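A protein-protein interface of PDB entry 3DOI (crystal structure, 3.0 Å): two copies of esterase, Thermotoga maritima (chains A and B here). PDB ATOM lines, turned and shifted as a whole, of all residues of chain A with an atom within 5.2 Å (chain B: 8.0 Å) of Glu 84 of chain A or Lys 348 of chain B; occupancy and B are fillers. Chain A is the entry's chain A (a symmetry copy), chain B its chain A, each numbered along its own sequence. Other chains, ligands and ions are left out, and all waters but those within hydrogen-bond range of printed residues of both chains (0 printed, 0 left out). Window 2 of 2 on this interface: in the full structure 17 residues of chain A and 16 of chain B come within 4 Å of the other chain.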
ATOM      1  N   LYS A  14     -10.208  24.897  27.644  1.00  0.00           N
ATOM      2  CA  LYS A  14     -10.159  24.500  26.265  1.00  0.00           C
ATOM      3  C   LYS A  14     -10.551  25.756  25.541  1.00  0.00           C
ATOM      4  O   LYS A  14     -11.241  26.584  26.112  1.00  0.00           O
ATOM      5  CB  LYS A  14     -11.155  23.374  26.039  1.00  0.00           C
ATOM      6  CG  LYS A  14     -11.184  22.758  24.669  1.00  0.00           C
ATOM      7  CD  LYS A  14     -12.597  22.256  24.406  1.00  0.00           C
ATOM      8  CE  LYS A  14     -12.681  21.209  23.335  1.00  0.00           C
ATOM      9  NZ  LYS A  14     -12.213  19.900  23.861  1.00  0.00           N
ATOM     10  N   CYS A  23     -13.643  24.134  31.292  1.00  0.00           N
ATOM     11  CA  CYS A  23     -14.533  23.189  30.670  1.00  0.00           C
ATOM     12  C   CYS A  23     -14.699  21.928  31.492  1.00  0.00           C
ATOM     13  O   CYS A  23     -15.698  21.221  31.337  1.00  0.00           O
ATOM     14  CB  CYS A  23     -14.081  22.892  29.236  1.00  0.00           C
ATOM     15  SG  CYS A  23     -12.863  21.561  29.055  1.00  0.00           S
ATOM     16  N   ALA A  24     -13.725  21.640  32.356  1.00  0.00           N
ATOM     17  CA  ALA A  24     -13.855  20.529  33.310  1.00  0.00           C
ATOM     18  C   ALA A  24     -12.985  20.709  34.548  1.00  0.00           C
ATOM     19  O   ALA A  24     -12.126  21.590  34.594  1.00  0.00           O
ATOM     20  CB  ALA A  24     -13.557  19.201  32.647  1.00  0.00           C
ATOM     21  N   VAL A  25     -13.220  19.877  35.561  1.00  0.00           N
ATOM     22  CA  VAL A  25     -12.377  19.858  36.766  1.00  0.00           C
ATOM     23  C   VAL A  25     -11.986  18.419  37.054  1.00  0.00           C
ATOM     24  O   VAL A  25     -12.840  17.524  37.060  1.00  0.00           O
ATOM     25  CB  VAL A  25     -13.084  20.480  37.991  1.00  0.00           C
ATOM     26  CG1 VAL A  25     -12.332  20.146  39.223  1.00  0.00           C
ATOM     27  CG2 VAL A  25     -13.221  21.996  37.845  1.00  0.00           C
ATOM     28  N   THR A  57     -22.420  24.397  35.972  1.00  0.00           N
ATOM     29  CA  THR A  57     -23.274  23.227  35.891  1.00  0.00           C
ATOM     30  C   THR A  57     -22.547  22.029  35.302  1.00  0.00           C
ATOM     31  O   THR A  57     -21.967  22.120  34.243  1.00  0.00           O
ATOM     32  CB  THR A  57     -24.639  23.547  35.202  1.00  0.00           C
ATOM     33  OG1 THR A  57     -24.883  22.639  34.130  1.00  0.00           O
ATOM     34  CG2 THR A  57     -24.688  24.966  34.675  1.00  0.00           C
ATOM     35  N   ILE A  58     -22.567  20.920  36.025  1.00  0.00           N
ATOM     36  CA  ILE A  58     -21.842  19.698  35.674  1.00  0.00           C
ATOM     37  C   ILE A  58     -22.697  18.818  34.784  1.00  0.00           C
ATOM     38  O   ILE A  58     -23.745  18.340  35.194  1.00  0.00           O
ATOM     39  CB  ILE A  58     -21.497  18.876  36.947  1.00  0.00           C
ATOM     40  CG1 ILE A  58     -20.771  19.762  37.954  1.00  0.00           C
ATOM     41  CG2 ILE A  58     -20.713  17.612  36.592  1.00  0.00           C
ATOM     42  CD1 ILE A  58     -21.108  19.445  39.366  1.00  0.00           C
ATOM     43  N   THR A  59     -22.227  18.569  33.572  1.00  0.00           N
ATOM     44  CA  THR A  59     -22.987  17.788  32.600  1.00  0.00           C
ATOM     45  C   THR A  59     -22.786  16.257  32.719  1.00  0.00           C
ATOM     46  O   THR A  59     -23.765  15.517  32.779  1.00  0.00           O
ATOM     47  CB  THR A  59     -22.714  18.278  31.163  1.00  0.00           C
ATOM     48  OG1 THR A  59     -21.299  18.348  30.932  1.00  0.00           O
ATOM     49  CG2 THR A  59     -23.279  19.643  30.977  1.00  0.00           C
ATOM     50  N   LYS A  60     -21.533  15.816  32.752  1.00  0.00           N
ATOM     51  CA  LYS A  60     -21.222  14.408  32.975  1.00  0.00           C
ATOM     52  C   LYS A  60     -20.413  14.216  34.254  1.00  0.00           C
ATOM     53  O   LYS A  60     -20.000  15.186  34.891  1.00  0.00           O
ATOM     54  CB  LYS A  60     -20.459  13.832  31.779  1.00  0.00           C
ATOM     55  CG  LYS A  60     -20.968  14.311  30.430  1.00  0.00           C
ATOM     56  CD  LYS A  60     -22.430  13.946  30.229  1.00  0.00           C
ATOM     57  CE  LYS A  60     -22.652  13.271  28.886  1.00  0.00           C
ATOM     58  NZ  LYS A  60     -22.258  14.150  27.751  1.00  0.00           N
ATOM     59  N   TYR A  62     -17.217  11.078  35.252  1.00  0.00           N
ATOM     60  CA  TYR A  62     -16.592   9.790  34.934  1.00  0.00           C
ATOM     61  C   TYR A  62     -15.157   9.682  35.459  1.00  0.00           C
ATOM     62  O   TYR A  62     -14.526  10.685  35.860  1.00  0.00           O
ATOM     63  CB  TYR A  62     -16.639   9.516  33.412  1.00  0.00           C
ATOM     64  CG  TYR A  62     -16.026  10.606  32.555  1.00  0.00           C
ATOM     65  CD1 TYR A  62     -16.816  11.594  31.966  1.00  0.00           C
ATOM     66  CD2 TYR A  62     -14.665  10.657  32.346  1.00  0.00           C
ATOM     67  CE1 TYR A  62     -16.252  12.606  31.204  1.00  0.00           C
ATOM     68  CE2 TYR A  62     -14.095  11.665  31.586  1.00  0.00           C
ATOM     69  CZ  TYR A  62     -14.890  12.621  31.026  1.00  0.00           C
ATOM     70  OH  TYR A  62     -14.299  13.578  30.275  1.00  0.00           O
ATOM     71  N   LEU A  69      -9.698  14.575  29.521  1.00  0.00           N
ATOM     72  CA  LEU A  69     -11.118  14.386  29.262  1.00  0.00           C
ATOM     73  C   LEU A  69     -11.418  13.021  28.592  1.00  0.00           C
ATOM     74  O   LEU A  69     -12.512  12.812  28.085  1.00  0.00           O
ATOM     75  CB  LEU A  69     -11.676  15.540  28.402  1.00  0.00           C
ATOM     76  CG  LEU A  69     -11.491  17.043  28.713  1.00  0.00           C
ATOM     77  CD1 LEU A  69     -12.627  17.836  28.064  1.00  0.00           C
ATOM     78  CD2 LEU A  69     -11.421  17.384  30.205  1.00  0.00           C
ATOM     79  N   VAL A  82     -13.264  13.013  36.724  1.00  0.00           N
ATOM     80  CA  VAL A  82     -13.543  14.133  35.819  1.00  0.00           C
ATOM     81  C   VAL A  82     -14.912  14.735  36.060  1.00  0.00           C
ATOM     82  O   VAL A  82     -15.906  14.026  36.102  1.00  0.00           O
ATOM     83  CB  VAL A  82     -13.446  13.699  34.331  1.00  0.00           C
ATOM     84  CG1 VAL A  82     -14.127  14.709  33.421  1.00  0.00           C
ATOM     85  CG2 VAL A  82     -11.989  13.553  33.916  1.00  0.00           C
ATOM     86  N   LEU A  83     -14.964  16.047  36.213  1.00  0.00           N
ATOM     87  CA  LEU A  83     -16.246  16.703  36.273  1.00  0.00           C
ATOM     88  C   LEU A  83     -16.382  17.647  35.093  1.00  0.00           C
ATOM     89  O   LEU A  83     -15.868  18.774  35.121  1.00  0.00           O
ATOM     90  CB  LEU A  83     -16.435  17.453  37.596  1.00  0.00           C
ATOM     91  CG  LEU A  83     -16.245  16.731  38.937  1.00  0.00           C
ATOM     92  CD1 LEU A  83     -16.295  17.749  40.056  1.00  0.00           C
ATOM     93  CD2 LEU A  83     -17.251  15.625  39.159  1.00  0.00           C
ATOM     94  N   GLU A  84     -17.075  17.179  34.056  1.00  0.00           N
ATOM     95  CA  GLU A  84     -17.281  17.975  32.859  1.00  0.00           C
ATOM     96  C   GLU A  84     -18.392  19.016  33.050  1.00  0.00           C
ATOM     97  O   GLU A  84     -19.469  18.698  33.542  1.00  0.00           O
ATOM     98  CB  GLU A  84     -17.544  17.078  31.655  1.00  0.00           C
ATOM     99  CG  GLU A  84     -18.105  17.866  30.473  1.00  0.00           C
ATOM    100  CD  GLU A  84     -18.323  17.017  29.231  1.00  0.00           C
ATOM    101  OE1 GLU A  84     -17.572  16.006  29.059  1.00  0.00           O
ATOM    102  OE2 GLU A  84     -19.229  17.398  28.426  1.00  0.00           O
ATOM    103  N   LEU A  85     -18.115  20.253  32.649  1.00  0.00           N
ATOM    104  CA  LEU A  85     -19.005  21.378  32.926  1.00  0.00           C
ATOM    105  C   LEU A  85     -19.627  21.942  31.685  1.00  0.00           C
ATOM    106  O   LEU A  85     -19.009  21.919  30.633  1.00  0.00           O
ATOM    107  CB  LEU A  85     -18.229  22.508  33.573  1.00  0.00           C
ATOM    108  CG  LEU A  85     -17.154  22.149  34.578  1.00  0.00           C
ATOM    109  CD1 LEU A  85     -16.482  23.459  35.025  1.00  0.00           C
ATOM    110  CD2 LEU A  85     -17.786  21.374  35.743  1.00  0.00           C
ATOM    111  N   SER A  86     -20.835  22.486  31.807  1.00  0.00           N
ATOM    112  CA  SER A  86     -21.535  23.005  30.629  1.00  0.00           C
ATOM    113  C   SER A  86     -20.846  24.212  30.121  1.00  0.00           C
ATOM    114  O   SER A  86     -20.564  25.141  30.858  1.00  0.00           O
ATOM    115  CB  SER A  86     -23.007  23.369  30.873  1.00  0.00           C
ATOM    116  OG  SER A  86     -23.576  24.003  29.711  1.00  0.00           O
ATOM    117  N   ARG A 207      -6.831  16.656  15.136  1.00  0.00           N
ATOM    118  CA  ARG A 207      -7.504  16.382  13.860  1.00  0.00           C
ATOM    119  C   ARG A 207      -6.792  16.941  12.628  1.00  0.00           C
ATOM    120  O   ARG A 207      -6.926  16.379  11.537  1.00  0.00           O
ATOM    121  CB  ARG A 207      -8.956  16.864  13.877  1.00  0.00           C
ATOM    122  CG  ARG A 207      -9.116  18.369  13.983  1.00  0.00           C
ATOM    123  CD  ARG A 207     -10.568  18.752  13.875  1.00  0.00           C
ATOM    124  NE  ARG A 207     -11.397  17.878  14.695  1.00  0.00           N
ATOM    125  CZ  ARG A 207     -11.653  18.101  15.972  1.00  0.00           C
ATOM    126  NH1 ARG A 207     -11.144  19.184  16.553  1.00  0.00           N
ATOM    127  NH2 ARG A 207     -12.412  17.254  16.663  1.00  0.00           N
ATOM    128  N   ALA B 316     -15.520  10.122  15.782  1.00  0.00           N
ATOM    129  CA  ALA B 316     -15.852  11.303  16.602  1.00  0.00           C
ATOM    130  C   ALA B 316     -14.848  11.386  17.724  1.00  0.00           C
ATOM    131  O   ALA B 316     -14.450  10.359  18.262  1.00  0.00           O
ATOM    132  CB  ALA B 316     -17.268  11.256  17.148  1.00  0.00           C
ATOM    133  N   GLU B 317     -14.433  12.600  18.067  1.00  0.00           N
ATOM    134  CA  GLU B 317     -13.352  12.809  19.037  1.00  0.00           C
ATOM    135  C   GLU B 317     -13.635  12.120  20.383  1.00  0.00           C
ATOM    136  O   GLU B 317     -12.768  11.458  20.985  1.00  0.00           O
ATOM    137  CB  GLU B 317     -13.102  14.310  19.213  1.00  0.00           C
ATOM    138  CG  GLU B 317     -11.913  14.650  20.098  1.00  0.00           C
ATOM    139  CD  GLU B 317     -12.252  14.662  21.593  1.00  0.00           C
ATOM    140  OE1 GLU B 317     -13.392  14.323  21.999  1.00  0.00           O
ATOM    141  OE2 GLU B 317     -11.358  15.016  22.376  1.00  0.00           O
ATOM    142  N   ASP B 318     -14.870  12.277  20.832  1.00  0.00           N
ATOM    143  CA  ASP B 318     -15.298  11.745  22.102  1.00  0.00           C
ATOM    144  C   ASP B 318     -16.026  10.386  22.029  1.00  0.00           C
ATOM    145  O   ASP B 318     -16.894  10.121  22.864  1.00  0.00           O
ATOM    146  CB  ASP B 318     -16.124  12.804  22.848  1.00  0.00           C
ATOM    147  CG  ASP B 318     -17.363  13.278  22.074  1.00  0.00           C
ATOM    148  OD1 ASP B 318     -17.568  12.949  20.877  1.00  0.00           O
ATOM    149  OD2 ASP B 318     -18.161  14.000  22.699  1.00  0.00           O
ATOM    150  N   ASP B 319     -15.686   9.535  21.047  1.00  0.00           N
ATOM    151  CA  ASP B 319     -16.198   8.152  21.009  1.00  0.00           C
ATOM    152  C   ASP B 319     -15.543   7.374  22.153  1.00  0.00           C
ATOM    153  O   ASP B 319     -14.318   7.289  22.192  1.00  0.00           O
ATOM    154  CB  ASP B 319     -15.894   7.486  19.654  1.00  0.00           C
ATOM    155  CG  ASP B 319     -16.350   5.998  19.576  1.00  0.00           C
ATOM    156  OD1 ASP B 319     -16.757   5.398  20.586  1.00  0.00           O
ATOM    157  OD2 ASP B 319     -16.293   5.417  18.467  1.00  0.00           O
ATOM    158  N   GLU B 345     -12.662  14.336  11.631  1.00  0.00           N
ATOM    159  CA  GLU B 345     -12.860  13.936  13.020  1.00  0.00           C
ATOM    160  C   GLU B 345     -13.802  14.874  13.757  1.00  0.00           C
ATOM    161  O   GLU B 345     -13.400  15.989  14.108  1.00  0.00           O
ATOM    162  CB  GLU B 345     -11.540  13.949  13.744  1.00  0.00           C
ATOM    163  CG  GLU B 345     -11.681  13.569  15.190  1.00  0.00           C
ATOM    164  CD  GLU B 345     -10.371  13.557  15.938  1.00  0.00           C
ATOM    165  OE1 GLU B 345      -9.446  12.783  15.584  1.00  0.00           O
ATOM    166  OE2 GLU B 345     -10.280  14.325  16.906  1.00  0.00           O
ATOM    167  N   TYR B 346     -15.038  14.434  14.012  1.00  0.00           N
ATOM    168  CA  TYR B 346     -16.080  15.298  14.657  1.00  0.00           C
ATOM    169  C   TYR B 346     -15.732  15.792  16.079  1.00  0.00           C
ATOM    170  O   TYR B 346     -15.292  15.015  16.944  1.00  0.00           O
ATOM    171  CB  TYR B 346     -17.460  14.616  14.685  1.00  0.00           C
ATOM    172  CG  TYR B 346     -17.894  14.009  13.373  1.00  0.00           C
ATOM    173  CD1 TYR B 346     -18.423  14.810  12.352  1.00  0.00           C
ATOM    174  CD2 TYR B 346     -17.776  12.628  13.152  1.00  0.00           C
ATOM    175  CE1 TYR B 346     -18.814  14.263  11.125  1.00  0.00           C
ATOM    176  CE2 TYR B 346     -18.166  12.051  11.936  1.00  0.00           C
ATOM    177  CZ  TYR B 346     -18.687  12.876  10.912  1.00  0.00           C
ATOM    178  OH  TYR B 346     -19.097  12.314   9.696  1.00  0.00           O
ATOM    179  N   GLU B 347     -15.949  17.086  16.301  1.00  0.00           N
ATOM    180  CA  GLU B 347     -15.630  17.778  17.559  1.00  0.00           C
ATOM    181  C   GLU B 347     -16.335  17.208  18.793  1.00  0.00           C
ATOM    182  O   GLU B 347     -17.509  16.802  18.709  1.00  0.00           O
ATOM    183  CB  GLU B 347     -16.048  19.237  17.422  1.00  0.00           C
ATOM    184  CG  GLU B 347     -15.522  19.941  16.209  1.00  0.00           C
ATOM    185  CD  GLU B 347     -15.206  21.361  16.549  1.00  0.00           C
ATOM    186  OE1 GLU B 347     -15.479  22.256  15.721  1.00  0.00           O
ATOM    187  OE2 GLU B 347     -14.701  21.587  17.679  1.00  0.00           O
ATOM    188  N   LYS B 348     -15.646  17.210  19.942  1.00  0.00           N
ATOM    189  CA  LYS B 348     -16.283  16.820  21.213  1.00  0.00           C
ATOM    190  C   LYS B 348     -17.603  17.582  21.360  1.00  0.00           C
ATOM    191  O   LYS B 348     -17.657  18.797  21.116  1.00  0.00           O
ATOM    192  CB  LYS B 348     -15.378  17.102  22.412  1.00  0.00           C
ATOM    193  CG  LYS B 348     -15.893  16.523  23.751  1.00  0.00           C
ATOM    194  CD  LYS B 348     -14.868  16.722  24.903  1.00  0.00           C
ATOM    195  CE  LYS B 348     -15.394  16.194  26.260  1.00  0.00           C
ATOM    196  NZ  LYS B 348     -15.082  14.731  26.507  1.00  0.00           N
ATOM    197  N   GLY B 349     -18.669  16.872  21.708  1.00  0.00           N
ATOM    198  CA  GLY B 349     -19.981  17.484  21.780  1.00  0.00           C
ATOM    199  C   GLY B 349     -20.792  17.412  20.494  1.00  0.00           C
ATOM    200  O   GLY B 349     -21.984  17.103  20.551  1.00  0.00           O
ATOM    201  N   PHE B 350     -20.165  17.684  19.342  1.00  0.00           N
ATOM    202  CA  PHE B 350     -20.893  17.788  18.054  1.00  0.00           C
ATOM    203  C   PHE B 350     -21.961  16.732  17.877  1.00  0.00           C
ATOM    204  O   PHE B 350     -23.056  17.005  17.379  1.00  0.00           O
ATOM    205  CB  PHE B 350     -19.959  17.718  16.845  1.00  0.00           C
ATOM    206  CG  PHE B 350     -20.679  17.503  15.521  1.00  0.00           C
ATOM    207  CD1 PHE B 350     -21.116  18.585  14.765  1.00  0.00           C
ATOM    208  CD2 PHE B 350     -20.915  16.220  15.032  1.00  0.00           C
ATOM    209  CE1 PHE B 350     -21.773  18.399  13.547  1.00  0.00           C
ATOM    210  CE2 PHE B 350     -21.581  16.023  13.817  1.00  0.00           C
ATOM    211  CZ  PHE B 350     -22.009  17.117  13.079  1.00  0.00           C
ATOM    212  N   MET B 351     -21.633  15.510  18.256  1.00  0.00           N
ATOM    213  CA  MET B 351     -22.567  14.429  18.098  1.00  0.00           C
ATOM    214  C   MET B 351     -23.757  14.647  19.028  1.00  0.00           C
ATOM    215  O   MET B 351     -24.893  14.813  18.574  1.00  0.00           O
ATOM    216  CB  MET B 351     -21.858  13.115  18.386  1.00  0.00           C
ATOM    217  CG  MET B 351     -20.740  12.841  17.415  1.00  0.00           C
ATOM    218  SD  MET B 351     -21.436  12.401  15.833  1.00  0.00           S
ATOM    219  CE  MET B 351     -22.154  10.840  16.308  1.00  0.00           C
ATOM    220  N   GLU B 352     -23.470  14.666  20.330  1.00  0.00           N
ATOM    221  CA  GLU B 352     -24.474  14.876  21.382  1.00  0.00           C
ATOM    222  C   GLU B 352     -25.427  16.000  20.994  1.00  0.00           C
ATOM    223  O   GLU B 352     -26.631  15.788  20.917  1.00  0.00           O
ATOM    224  CB  GLU B 352     -23.770  15.201  22.706  1.00  0.00           C
ATOM    225  CG  GLU B 352     -22.838  14.091  23.229  1.00  0.00           C
ATOM    226  CD  GLU B 352     -23.606  12.932  23.922  1.00  0.00           C
ATOM    227  OE1 GLU B 352     -24.786  12.659  23.562  1.00  0.00           O
ATOM    228  OE2 GLU B 352     -23.009  12.291  24.835  1.00  0.00           O
ATOM    229  N   LYS B 353     -24.855  17.185  20.751  1.00  0.00           N
ATOM    230  CA  LYS B 353     -25.514  18.346  20.146  1.00  0.00           C
ATOM    231  C   LYS B 353     -26.594  18.001  19.096  1.00  0.00           C
ATOM    232  O   LYS B 353     -27.614  18.664  19.039  1.00  0.00           O
ATOM    233  CB  LYS B 353     -24.420  19.282  19.587  1.00  0.00           C
ATOM    234  CG  LYS B 353     -24.860  20.472  18.704  1.00  0.00           C
ATOM    235  CD  LYS B 353     -23.711  21.532  18.560  1.00  0.00           C
ATOM    236  CE  LYS B 353     -24.169  22.884  17.935  1.00  0.00           C
ATOM    237  NZ  LYS B 353     -24.629  22.796  16.497  1.00  0.00           N
ATOM    238  N   PRO B 358     -22.002   9.579  20.926  1.00  0.00           N
ATOM    239  CA  PRO B 358     -20.771   9.930  20.169  1.00  0.00           C
ATOM    240  C   PRO B 358     -20.120   8.740  19.436  1.00  0.00           C
ATOM    241  O   PRO B 358     -19.347   8.947  18.521  1.00  0.00           O
ATOM    242  CB  PRO B 358     -19.840  10.549  21.228  1.00  0.00           C
ATOM    243  CG  PRO B 358     -20.390  10.122  22.552  1.00  0.00           C
ATOM    244  CD  PRO B 358     -21.875   9.873  22.371  1.00  0.00           C
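The side-chain carboxylate (OE2) of Glu 345 of chain B is in salt-bridge range of the guanidinium group (NH2) of Arg 207 of chain A (3.6 Å).
The side-chain amino group (NZ) of Lys 348 of chain B is in salt-bridge range of the side-chain carboxylate (OE1) of Glu 84 of chain A (3.8 Å).
OE2 of Glu 352 of chain B lies within salt-bridge range of NZ of Lys 60 of chain A (3.5 Å).
The backbone NH of Glu 317 of chain B is in hydrogen-bond range of the backbone carbonyl oxygen of Tyr 346 of chain B (2.8 Å).
N of Thr 59 of chain A lies within hydrogen-bond range of O of Glu 84 of chain A.
The backbone carbonyl oxygen of Leu 69 of chain A sits at hydrogen-bond distance from the side-chain hydroxyl of Tyr 62 of chain A (2.9 Å).
Among the printed residues, merely in contact across the chains: Leu 69 of chain A with Lys 348 of chain B, Arg 207 of chain A with Glu 317 of chain B, Arg 207 of chain A with Tyr 346 of chain B and Arg 207 of chain A with Glu 347 of chain B.
Glu 84 of chain A touches just one residue of chain B: Lys 348.
Of the printed residues of chain A, Lys 348 of chain B touches Leu 69 (3.6 Å) and Glu 84 (3.6 Å).
Of the printed residues of chain A, Glu 345 of chain B touches Arg 207 (2.8 Å).
Printed residues of chain A within 4 Å of Tyr 346 of chain B: Arg 207 (3.7 Å).
Ile 58 of chain A touches none of the printed residues of chain B.
The nearest printed residue of chain B that does not touch Glu 84 of chain A is Gly 349 of chain B (6.7 Å).
The nearest printed residue of chain A that does not touch Lys 348 of chain B is Tyr 62 of chain A (4.02 Å).
Printed residues of chain B that touch a printed residue of chain A: Glu 317, Glu 345, Tyr 346, Glu 347, Lys 348 and Glu 352.
Printed residues of chain A that touch a printed residue of chain B: Lys 60, Leu 69, Glu 84 and Arg 207.
No position is printed for both chains.
Of the 7 pairs that touch across the chains among the printed residues, none has its exchanged pair printed and touching as well.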
